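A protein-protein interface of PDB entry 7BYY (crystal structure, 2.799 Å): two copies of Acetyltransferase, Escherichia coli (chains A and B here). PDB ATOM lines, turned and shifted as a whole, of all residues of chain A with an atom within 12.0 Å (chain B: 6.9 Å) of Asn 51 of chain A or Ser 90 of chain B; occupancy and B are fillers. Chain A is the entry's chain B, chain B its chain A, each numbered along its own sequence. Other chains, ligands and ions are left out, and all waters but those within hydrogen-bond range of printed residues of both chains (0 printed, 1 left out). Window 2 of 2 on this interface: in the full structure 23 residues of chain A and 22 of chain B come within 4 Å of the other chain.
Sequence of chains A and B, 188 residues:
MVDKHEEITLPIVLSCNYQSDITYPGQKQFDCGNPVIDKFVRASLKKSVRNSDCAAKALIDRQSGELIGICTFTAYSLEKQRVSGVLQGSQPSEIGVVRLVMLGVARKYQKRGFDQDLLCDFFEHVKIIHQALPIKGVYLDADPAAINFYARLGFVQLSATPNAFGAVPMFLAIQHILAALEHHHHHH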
ATOM      1  N   TYR A  18     -36.984 -14.802  29.482  1.00  0.00           N
ATOM      2  CA  TYR A  18     -37.327 -14.566  28.086  1.00  0.00           C
ATOM      3  C   TYR A  18     -37.184 -15.846  27.277  1.00  0.00           C
ATOM      4  O   TYR A  18     -36.091 -16.412  27.173  1.00  0.00           O
ATOM      5  CB  TYR A  18     -36.447 -13.463  27.503  1.00  0.00           C
ATOM      6  CG  TYR A  18     -36.823 -13.072  26.090  1.00  0.00           C
ATOM      7  CD1 TYR A  18     -36.232 -13.693  24.995  1.00  0.00           C
ATOM      8  CD2 TYR A  18     -37.768 -12.083  25.852  1.00  0.00           C
ATOM      9  CE1 TYR A  18     -36.574 -13.340  23.704  1.00  0.00           C
ATOM     10  CE2 TYR A  18     -38.115 -11.721  24.564  1.00  0.00           C
ATOM     11  CZ  TYR A  18     -37.516 -12.354  23.494  1.00  0.00           C
ATOM     12  OH  TYR A  18     -37.860 -12.001  22.209  1.00  0.00           O
ATOM     13  N   GLN A  19     -38.293 -16.299  26.703  1.00  0.00           N
ATOM     14  CA  GLN A  19     -38.328 -17.496  25.876  1.00  0.00           C
ATOM     15  C   GLN A  19     -38.602 -17.096  24.433  1.00  0.00           C
ATOM     16  O   GLN A  19     -39.509 -16.301  24.167  1.00  0.00           O
ATOM     17  CB  GLN A  19     -39.388 -18.476  26.381  1.00  0.00           C
ATOM     18  CG  GLN A  19     -39.069 -19.068  27.744  1.00  0.00           C
ATOM     19  CD  GLN A  19     -40.065 -20.127  28.164  1.00  0.00           C
ATOM     20  OE1 GLN A  19     -41.241 -20.067  27.801  1.00  0.00           O
ATOM     21  NE2 GLN A  19     -39.599 -21.110  28.926  1.00  0.00           N
ATOM     22  N   SER A  20     -37.813 -17.650  23.509  1.00  0.00           N
ATOM     23  CA  SER A  20     -37.864 -17.238  22.111  1.00  0.00           C
ATOM     24  C   SER A  20     -39.095 -17.751  21.376  1.00  0.00           C
ATOM     25  O   SER A  20     -39.369 -17.278  20.269  1.00  0.00           O
ATOM     26  CB  SER A  20     -36.604 -17.706  21.381  1.00  0.00           C
ATOM     27  OG  SER A  20     -36.384 -19.093  21.577  1.00  0.00           O
ATOM     28  N   ASP A  21     -39.834 -18.700  21.951  1.00  0.00           N
ATOM     29  CA  ASP A  21     -41.038 -19.199  21.300  1.00  0.00           C
ATOM     30  C   ASP A  21     -42.235 -18.282  21.502  1.00  0.00           C
ATOM     31  O   ASP A  21     -43.164 -18.307  20.685  1.00  0.00           O
ATOM     32  CB  ASP A  21     -41.376 -20.601  21.813  1.00  0.00           C
ATOM     33  CG  ASP A  21     -40.148 -21.473  21.976  1.00  0.00           C
ATOM     34  OD1 ASP A  21     -39.905 -21.959  23.101  1.00  0.00           O
ATOM     35  OD2 ASP A  21     -39.422 -21.670  20.978  1.00  0.00           O
ATOM     36  N   PHE A  40     -31.443  -4.232  19.327  1.00  0.00           N
ATOM     37  CA  PHE A  40     -31.100  -5.599  19.698  1.00  0.00           C
ATOM     38  C   PHE A  40     -32.342  -6.378  20.110  1.00  0.00           C
ATOM     39  O   PHE A  40     -32.480  -7.563  19.778  1.00  0.00           O
ATOM     40  CB  PHE A  40     -30.069  -5.601  20.826  1.00  0.00           C
ATOM     41  CG  PHE A  40     -29.798  -6.966  21.394  1.00  0.00           C
ATOM     42  CD1 PHE A  40     -30.387  -7.370  22.580  1.00  0.00           C
ATOM     43  CD2 PHE A  40     -28.957  -7.848  20.735  1.00  0.00           C
ATOM     44  CE1 PHE A  40     -30.141  -8.626  23.099  1.00  0.00           C
ATOM     45  CE2 PHE A  40     -28.706  -9.105  21.248  1.00  0.00           C
ATOM     46  CZ  PHE A  40     -29.299  -9.494  22.432  1.00  0.00           C
ATOM     47  N   ALA A  43     -34.710  -7.354  16.790  1.00  0.00           N
ATOM     48  CA  ALA A  43     -34.373  -8.364  15.791  1.00  0.00           C
ATOM     49  C   ALA A  43     -33.440  -9.449  16.303  1.00  0.00           C
ATOM     50  O   ALA A  43     -33.558 -10.601  15.877  1.00  0.00           O
ATOM     51  CB  ALA A  43     -33.749  -7.689  14.561  1.00  0.00           C
ATOM     52  N   SER A  44     -32.518  -9.118  17.206  1.00  0.00           N
ATOM     53  CA  SER A  44     -31.446 -10.051  17.533  1.00  0.00           C
ATOM     54  C   SER A  44     -31.745 -10.912  18.755  1.00  0.00           C
ATOM     55  O   SER A  44     -31.369 -12.089  18.780  1.00  0.00           O
ATOM     56  CB  SER A  44     -30.139  -9.286  17.747  1.00  0.00           C
ATOM     57  OG  SER A  44     -29.839  -8.468  16.628  1.00  0.00           O
ATOM     58  N   LEU A  45     -32.418 -10.355  19.767  1.00  0.00           N
ATOM     59  CA  LEU A  45     -32.549 -11.047  21.047  1.00  0.00           C
ATOM     60  C   LEU A  45     -33.268 -12.383  20.895  1.00  0.00           C
ATOM     61  O   LEU A  45     -32.843 -13.390  21.474  1.00  0.00           O
ATOM     62  CB  LEU A  45     -33.279 -10.155  22.054  1.00  0.00           C
ATOM     63  CG  LEU A  45     -34.057 -10.807  23.203  1.00  0.00           C
ATOM     64  CD1 LEU A  45     -33.133 -11.572  24.149  1.00  0.00           C
ATOM     65  CD2 LEU A  45     -34.843  -9.757  23.967  1.00  0.00           C
ATOM     66  N   LYS A  46     -34.357 -12.415  20.123  1.00  0.00           N
ATOM     67  CA  LYS A  46     -35.099 -13.661  19.953  1.00  0.00           C
ATOM     68  C   LYS A  46     -34.210 -14.752  19.370  1.00  0.00           C
ATOM     69  O   LYS A  46     -34.219 -15.893  19.848  1.00  0.00           O
ATOM     70  CB  LYS A  46     -36.324 -13.427  19.068  1.00  0.00           C
ATOM     71  CG  LYS A  46     -37.156 -14.676  18.815  1.00  0.00           C
ATOM     72  CD  LYS A  46     -38.625 -14.333  18.596  1.00  0.00           C
ATOM     73  CE  LYS A  46     -39.269 -13.789  19.867  1.00  0.00           C
ATOM     74  NZ  LYS A  46     -40.737 -13.566  19.709  1.00  0.00           N
ATOM     75  N   LYS A  47     -33.419 -14.418  18.348  1.00  0.00           N
ATOM     76  CA  LYS A  47     -32.475 -15.392  17.813  1.00  0.00           C
ATOM     77  C   LYS A  47     -31.307 -15.615  18.763  1.00  0.00           C
ATOM     78  O   LYS A  47     -30.718 -16.703  18.774  1.00  0.00           O
ATOM     79  CB  LYS A  47     -31.964 -14.943  16.443  1.00  0.00           C
ATOM     80  CG  LYS A  47     -33.032 -14.347  15.537  1.00  0.00           C
ATOM     81  CD  LYS A  47     -32.612 -14.410  14.075  1.00  0.00           C
ATOM     82  CE  LYS A  47     -33.141 -13.218  13.296  1.00  0.00           C
ATOM     83  NZ  LYS A  47     -32.350 -11.982  13.565  1.00  0.00           N
ATOM     84  N   SER A  48     -30.973 -14.610  19.575  1.00  0.00           N
ATOM     85  CA  SER A  48     -29.808 -14.713  20.446  1.00  0.00           C
ATOM     86  C   SER A  48     -29.998 -15.788  21.510  1.00  0.00           C
ATOM     87  O   SER A  48     -29.052 -16.512  21.843  1.00  0.00           O
ATOM     88  CB  SER A  48     -29.518 -13.360  21.095  1.00  0.00           C
ATOM     89  OG  SER A  48     -28.264 -13.370  21.754  1.00  0.00           O
ATOM     90  N   VAL A  49     -31.209 -15.909  22.058  1.00  0.00           N
ATOM     91  CA  VAL A  49     -31.444 -16.915  23.089  1.00  0.00           C
ATOM     92  C   VAL A  49     -31.760 -18.280  22.496  1.00  0.00           C
ATOM     93  O   VAL A  49     -31.529 -19.301  23.157  1.00  0.00           O
ATOM     94  CB  VAL A  49     -32.566 -16.474  24.047  1.00  0.00           C
ATOM     95  CG1 VAL A  49     -32.201 -15.159  24.712  1.00  0.00           C
ATOM     96  CG2 VAL A  49     -33.887 -16.353  23.310  1.00  0.00           C
ATOM     97  N   ARG A  50     -32.280 -18.336  21.267  1.00  0.00           N
ATOM     98  CA  ARG A  50     -32.450 -19.624  20.604  1.00  0.00           C
ATOM     99  C   ARG A  50     -31.095 -20.251  20.306  1.00  0.00           C
ATOM    100  O   ARG A  50     -30.866 -21.432  20.596  1.00  0.00           O
ATOM    101  CB  ARG A  50     -33.271 -19.456  19.325  1.00  0.00           C
ATOM    102  CG  ARG A  50     -33.210 -20.652  18.388  1.00  0.00           C
ATOM    103  CD  ARG A  50     -34.376 -20.664  17.405  1.00  0.00           C
ATOM    104  NE  ARG A  50     -34.723 -19.325  16.935  1.00  0.00           N
ATOM    105  CZ  ARG A  50     -35.853 -18.693  17.240  1.00  0.00           C
ATOM    106  NH1 ARG A  50     -36.752 -19.276  18.021  1.00  0.00           N
ATOM    107  NH2 ARG A  50     -36.081 -17.474  16.766  1.00  0.00           N
ATOM    108  N   ASN A  51     -30.177 -19.467  19.739  1.00  0.00           N
ATOM    109  CA  ASN A  51     -28.787 -19.884  19.598  1.00  0.00           C
ATOM    110  C   ASN A  51     -28.046 -19.888  20.931  1.00  0.00           C
ATOM    111  O   ASN A  51     -26.873 -20.276  20.969  1.00  0.00           O
ATOM    112  CB  ASN A  51     -28.073 -18.972  18.595  1.00  0.00           C
ATOM    113  CG  ASN A  51     -26.798 -19.588  18.043  1.00  0.00           C
ATOM    114  OD1 ASN A  51     -25.697 -19.117  18.326  1.00  0.00           O
ATOM    115  ND2 ASN A  51     -26.944 -20.645  17.250  1.00  0.00           N
ATOM    116  N   SER A  52     -28.707 -19.465  22.011  1.00  0.00           N
ATOM    117  CA  SER A  52     -28.145 -19.481  23.361  1.00  0.00           C
ATOM    118  C   SER A  52     -26.842 -18.685  23.437  1.00  0.00           C
ATOM    119  O   SER A  52     -25.848 -19.127  24.016  1.00  0.00           O
ATOM    120  CB  SER A  52     -27.947 -20.916  23.857  1.00  0.00           C
ATOM    121  OG  SER A  52     -26.649 -21.388  23.547  1.00  0.00           O
ATOM    122  N   ASP A  53     -26.850 -17.497  22.832  1.00  0.00           N
ATOM    123  CA  ASP A  53     -25.741 -16.565  22.990  1.00  0.00           C
ATOM    124  C   ASP A  53     -25.824 -15.784  24.294  1.00  0.00           C
ATOM    125  O   ASP A  53     -24.857 -15.102  24.653  1.00  0.00           O
ATOM    126  CB  ASP A  53     -25.687 -15.588  21.810  1.00  0.00           C
ATOM    127  CG  ASP A  53     -25.487 -16.290  20.476  1.00  0.00           C
ATOM    128  OD1 ASP A  53     -25.945 -15.751  19.443  1.00  0.00           O
ATOM    129  OD2 ASP A  53     -24.875 -17.379  20.456  1.00  0.00           O
ATOM    130  N   CYS A  54     -26.947 -15.878  25.004  1.00  0.00           N
ATOM    131  CA  CYS A  54     -27.177 -15.187  26.266  1.00  0.00           C
ATOM    132  C   CYS A  54     -28.493 -15.678  26.845  1.00  0.00           C
ATOM    133  O   CYS A  54     -29.313 -16.280  26.144  1.00  0.00           O
ATOM    134  CB  CYS A  54     -27.224 -13.666  26.085  1.00  0.00           C
ATOM    135  SG  CYS A  54     -28.651 -13.079  25.126  1.00  0.00           S
ATOM    136  N   ALA A  55     -28.683 -15.419  28.132  1.00  0.00           N
ATOM    137  CA  ALA A  55     -29.987 -15.542  28.759  1.00  0.00           C
ATOM    138  C   ALA A  55     -30.554 -14.151  28.995  1.00  0.00           C
ATOM    139  O   ALA A  55     -29.823 -13.162  29.074  1.00  0.00           O
ATOM    140  CB  ALA A  55     -29.910 -16.313  30.080  1.00  0.00           C
ATOM    141  N   ALA A  56     -31.875 -14.077  29.102  1.00  0.00           N
ATOM    142  CA  ALA A  56     -32.540 -12.795  29.294  1.00  0.00           C
ATOM    143  C   ALA A  56     -33.664 -12.962  30.300  1.00  0.00           C
ATOM    144  O   ALA A  56     -34.561 -13.786  30.101  1.00  0.00           O
ATOM    145  CB  ALA A  56     -33.075 -12.249  27.967  1.00  0.00           C
ATOM    146  N   PHE A  73     -27.723 -11.375  30.034  1.00  0.00           N
ATOM    147  CA  PHE A  73     -26.498 -11.711  30.745  1.00  0.00           C
ATOM    148  C   PHE A  73     -25.885 -12.959  30.129  1.00  0.00           C
ATOM    149  O   PHE A  73     -26.565 -13.747  29.464  1.00  0.00           O
ATOM    150  CB  PHE A  73     -26.750 -11.916  32.244  1.00  0.00           C
ATOM    151  CG  PHE A  73     -27.845 -12.896  32.550  1.00  0.00           C
ATOM    152  CD1 PHE A  73     -29.170 -12.489  32.583  1.00  0.00           C
ATOM    153  CD2 PHE A  73     -27.551 -14.223  32.809  1.00  0.00           C
ATOM    154  CE1 PHE A  73     -30.184 -13.390  32.864  1.00  0.00           C
ATOM    155  CE2 PHE A  73     -28.557 -15.129  33.091  1.00  0.00           C
ATOM    156  CZ  PHE A  73     -29.876 -14.711  33.119  1.00  0.00           C
ATOM    157  N   THR A  74     -24.587 -13.135  30.366  1.00  0.00           N
ATOM    158  CA  THR A  74     -23.847 -14.224  29.749  1.00  0.00           C
ATOM    159  C   THR A  74     -22.728 -14.679  30.672  1.00  0.00           C
ATOM    160  O   THR A  74     -22.339 -13.976  31.610  1.00  0.00           O
ATOM    161  CB  THR A  74     -23.258 -13.811  28.395  1.00  0.00           C
ATOM    162  OG1 THR A  74     -22.694 -14.959  27.747  1.00  0.00           O
ATOM    163  CG2 THR A  74     -22.167 -12.766  28.592  1.00  0.00           C
ATOM    164  N   ALA A  75     -22.211 -15.873  30.387  1.00  0.00           N
ATOM    165  CA  ALA A  75     -21.027 -16.374  31.067  1.00  0.00           C
ATOM    166  C   ALA A  75     -19.794 -15.676  30.508  1.00  0.00           C
ATOM    167  O   ALA A  75     -19.627 -15.572  29.289  1.00  0.00           O
ATOM    168  CB  ALA A  75     -20.911 -17.888  30.898  1.00  0.00           C
ATOM    169  N   LEU B  87     -17.259 -24.572  16.456  1.00  0.00           N
ATOM    170  CA  LEU B  87     -18.568 -23.951  16.662  1.00  0.00           C
ATOM    171  C   LEU B  87     -19.032 -23.397  15.322  1.00  0.00           C
ATOM    172  O   LEU B  87     -18.526 -22.375  14.854  1.00  0.00           O
ATOM    173  CB  LEU B  87     -18.503 -22.857  17.721  1.00  0.00           C
ATOM    174  CG  LEU B  87     -18.932 -23.281  19.128  1.00  0.00           C
ATOM    175  CD1 LEU B  87     -18.912 -22.096  20.076  1.00  0.00           C
ATOM    176  CD2 LEU B  87     -20.310 -23.939  19.116  1.00  0.00           C
ATOM    177  N   GLN B  88     -19.995 -24.066  14.697  1.00  0.00           N
ATOM    178  CA  GLN B  88     -20.408 -23.675  13.362  1.00  0.00           C
ATOM    179  C   GLN B  88     -21.507 -22.627  13.438  1.00  0.00           C
ATOM    180  O   GLN B  88     -22.233 -22.508  14.434  1.00  0.00           O
ATOM    181  CB  GLN B  88     -20.909 -24.883  12.583  1.00  0.00           C
ATOM    182  CG  GLN B  88     -19.975 -26.107  12.551  1.00  0.00           C
ATOM    183  CD  GLN B  88     -18.502 -25.816  12.259  1.00  0.00           C
ATOM    184  OE1 GLN B  88     -17.795 -25.145  13.019  1.00  0.00           O
ATOM    185  NE2 GLN B  88     -18.034 -26.348  11.142  1.00  0.00           N
ATOM    186  N   GLY B  89     -21.637 -21.875  12.354  1.00  0.00           N
ATOM    187  CA  GLY B  89     -22.630 -20.825  12.310  1.00  0.00           C
ATOM    188  C   GLY B  89     -22.103 -19.540  12.900  1.00  0.00           C
ATOM    189  O   GLY B  89     -20.966 -19.443  13.369  1.00  0.00           O
ATOM    190  N   SER B  90     -22.961 -18.526  12.866  1.00  0.00           N
ATOM    191  CA  SER B  90     -22.612 -17.229  13.423  1.00  0.00           C
ATOM    192  C   SER B  90     -22.483 -17.326  14.938  1.00  0.00           C
ATOM    193  O   SER B  90     -23.379 -17.835  15.619  1.00  0.00           O
ATOM    194  CB  SER B  90     -23.665 -16.188  13.041  1.00  0.00           C
ATOM    195  OG  SER B  90     -24.969 -16.610  13.403  1.00  0.00           O
ATOM    196  N   GLN B  91     -21.363 -16.839  15.463  1.00  0.00           N
ATOM    197  CA  GLN B  91     -21.061 -16.902  16.883  1.00  0.00           C
ATOM    198  C   GLN B  91     -20.555 -15.554  17.374  1.00  0.00           C
ATOM    199  O   GLN B  91     -19.905 -14.818  16.624  1.00  0.00           O
ATOM    200  CB  GLN B  91     -20.013 -17.986  17.178  1.00  0.00           C
ATOM    201  CG  GLN B  91     -20.463 -19.400  16.825  1.00  0.00           C
ATOM    202  CD  GLN B  91     -21.508 -19.947  17.783  1.00  0.00           C
ATOM    203  OE1 GLN B  91     -21.392 -19.794  19.000  1.00  0.00           O
ATOM    204  NE2 GLN B  91     -22.532 -20.593  17.237  1.00  0.00           N
ATOM    205  N   PRO B  92     -20.842 -15.205  18.626  1.00  0.00           N
ATOM    206  CA  PRO B  92     -20.397 -13.912  19.157  1.00  0.00           C
ATOM    207  C   PRO B  92     -18.889 -13.874  19.362  1.00  0.00           C
ATOM    208  O   PRO B  92     -18.198 -14.895  19.372  1.00  0.00           O
ATOM    209  CB  PRO B  92     -21.147 -13.795  20.488  1.00  0.00           C
ATOM    210  CG  PRO B  92     -21.446 -15.205  20.876  1.00  0.00           C
ATOM    211  CD  PRO B  92     -21.672 -15.945  19.593  1.00  0.00           C
ATOM    212  N   HIS B 130     -26.270 -25.074  32.327  1.00  0.00           N
ATOM    213  CA  HIS B 130     -26.710 -24.520  31.052  1.00  0.00           C
ATOM    214  C   HIS B 130     -28.114 -23.936  31.138  1.00  0.00           C
ATOM    215  O   HIS B 130     -28.423 -22.963  30.439  1.00  0.00           O
ATOM    216  CB  HIS B 130     -26.649 -25.601  29.975  1.00  0.00           C
ATOM    217  CG  HIS B 130     -26.957 -25.101  28.598  1.00  0.00           C
ATOM    218  ND1 HIS B 130     -26.278 -24.051  28.018  1.00  0.00           N
ATOM    219  CD2 HIS B 130     -27.868 -25.511  27.684  1.00  0.00           C
ATOM    220  CE1 HIS B 130     -26.758 -23.837  26.805  1.00  0.00           C
ATOM    221  NE2 HIS B 130     -27.723 -24.710  26.579  1.00  0.00           N
ATOM    222  N   PRO B 134     -26.609 -19.864  29.911  1.00  0.00           N
ATOM    223  CA  PRO B 134     -26.257 -20.541  28.657  1.00  0.00           C
ATOM    224  C   PRO B 134     -24.756 -20.535  28.425  1.00  0.00           C
ATOM    225  O   PRO B 134     -24.078 -19.526  28.634  1.00  0.00           O
ATOM    226  CB  PRO B 134     -26.989 -19.719  27.586  1.00  0.00           C
ATOM    227  CG  PRO B 134     -28.009 -18.910  28.337  1.00  0.00           C
ATOM    228  CD  PRO B 134     -27.397 -18.646  29.676  1.00  0.00           C
ATOM    229  N   ILE B 135     -24.241 -21.684  27.995  1.00  0.00           N
ATOM    230  CA  ILE B 135     -22.839 -21.831  27.638  1.00  0.00           C
ATOM    231  C   ILE B 135     -22.761 -22.578  26.314  1.00  0.00           C
ATOM    232  O   ILE B 135     -23.691 -23.280  25.916  1.00  0.00           O
ATOM    233  CB  ILE B 135     -22.023 -22.545  28.741  1.00  0.00           C
ATOM    234  CG1 ILE B 135     -22.618 -23.914  29.091  1.00  0.00           C
ATOM    235  CG2 ILE B 135     -21.962 -21.684  29.989  1.00  0.00           C
ATOM    236  CD1 ILE B 135     -22.168 -25.050  28.197  1.00  0.00           C
ATOM    237  N   LYS B 136     -21.641 -22.397  25.617  1.00  0.00           N
ATOM    238  CA  LYS B 136     -21.466 -23.025  24.314  1.00  0.00           C
ATOM    239  C   LYS B 136     -20.929 -24.446  24.405  1.00  0.00           C
ATOM    240  O   LYS B 136     -21.145 -25.235  23.479  1.00  0.00           O
ATOM    241  CB  LYS B 136     -20.535 -22.179  23.442  1.00  0.00           C
ATOM    242  CG  LYS B 136     -21.158 -20.875  22.977  1.00  0.00           C
ATOM    243  CD  LYS B 136     -22.422 -21.136  22.181  1.00  0.00           C
ATOM    244  CE  LYS B 136     -23.072 -19.843  21.731  1.00  0.00           C
ATOM    245  NZ  LYS B 136     -24.115 -20.108  20.703  1.00  0.00           N
ATOM    246  N   GLN B 175     -24.341 -28.988  22.448  1.00  0.00           N
ATOM    247  CA  GLN B 175     -25.318 -29.815  21.747  1.00  0.00           C
ATOM    248  C   GLN B 175     -24.985 -31.298  21.879  1.00  0.00           C
ATOM    249  O   GLN B 175     -25.881 -32.132  22.055  1.00  0.00           O
ATOM    250  CB  GLN B 175     -25.389 -29.409  20.273  1.00  0.00           C
ATOM    251  CG  GLN B 175     -25.860 -27.977  20.035  1.00  0.00           C
ATOM    252  CD  GLN B 175     -24.739 -26.954  20.163  1.00  0.00           C
ATOM    253  OE1 GLN B 175     -23.561 -27.310  20.204  1.00  0.00           O
ATOM    254  NE2 GLN B 175     -25.106 -25.678  20.227  1.00  0.00           N
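Among the printed residues, pairs that only touch across the chains: Asn 51 of chain A with Ser 90 of chain B, Asn 51 of chain A with Gln 91 of chain B, Ser 52 of chain A with Pro 134 of chain B, Ser 52 of chain A with Lys 136 of chain B, Asp 53 of chain A with Pro 92 of chain B, Cys 54 of chain A with Pro 134 of chain B and Ala 55 of chain A with Pro 134 of chain B.
Ser 90 of chain B touches one residue of chain A.
No residue of chain A comes within 4 Å of Gly 89 of chain B.
Of chain A, only Asp 53 comes within 4 Å of Pro 92 of chain B.
Printed residues of chain A within 4 Å of Lys 136 of chain B: Asn 51, Ser 52 and Asp 53.
Of the printed residues of chain B, Cys 54 of chain A touches Pro 134.
Printed residues of chain A within 4 Å of Pro 134 of chain B: Ser 52 (3.8 Å), Cys 54 (3.6 Å) and Ala 55 (3.5 Å).
Of the printed residues of chain B, Ala 55 of chain A touches Pro 134.
Printed residues of chain B within 4 Å of Asp 53 of chain A: Pro 92 (3.6 Å) and Lys 136 (2.8 Å).
Val 49 of chain A touches none of the printed residues of chain B.
The nearest residue of chain B that does not touch Asn 51 of chain A is Pro 92 of chain B (5.3 Å).
No position is printed for both chains.
Of the 9 pairs that touch across the chains among the printed residues, none has its exchanged pair printed and touching as well.
Hydrophobic or aromatic side chains of chain B that line the printed part of chain A: Pro 92 and Pro 134.
Of the 22 printed residues of chain A, 5 touch a printed residue of chain B.
Among the printed residues, Asp or Glu carboxylates within 4 Å of a Lys or Arg side-chain nitrogen of the other chain: Asp 53 of chain A with Lys 136 of chain B (2.8 Å).
The side-chain hydroxyl (OG) of Ser 48 of chain A is in hydrogen-bond range of the side-chain sulfur (SG) of Cys 54 of chain A (3.4 Å).
O of Gln 88 of chain B sits at hydrogen-bond distance from NE2 of Gln 91 of chain B.
The backbone carbonyl oxygen of Ala 55 of chain A is in hydrogen-bond range of the backbone NH of Phe 73 of chain A (2.9 Å).
The backbone carbonyl oxygen of Ser 48 of chain A sits at hydrogen-bond distance from the backbone NH of Asp 53 of chain A (2.6 Å).
The side-chain amide oxygen of Gln 91 of chain B lies close to the side-chain amino group of Lys 136 of chain B (3.2 Å).
The side-chain carboxylate of Asp 53 of chain A lies close to the side-chain amide oxygen of Asn 51 of chain A, 2.9 Å away.
The side-chain carboxylate (OD2) of Asp 53 of chain A lies within salt-bridge range of the side-chain amino group (NZ) of Lys 136 of chain B (2.8 Å).
NZ of Lys 136 of chain B is in hydrogen-bond range of O of Asn 51 of chain A (2.8 Å).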
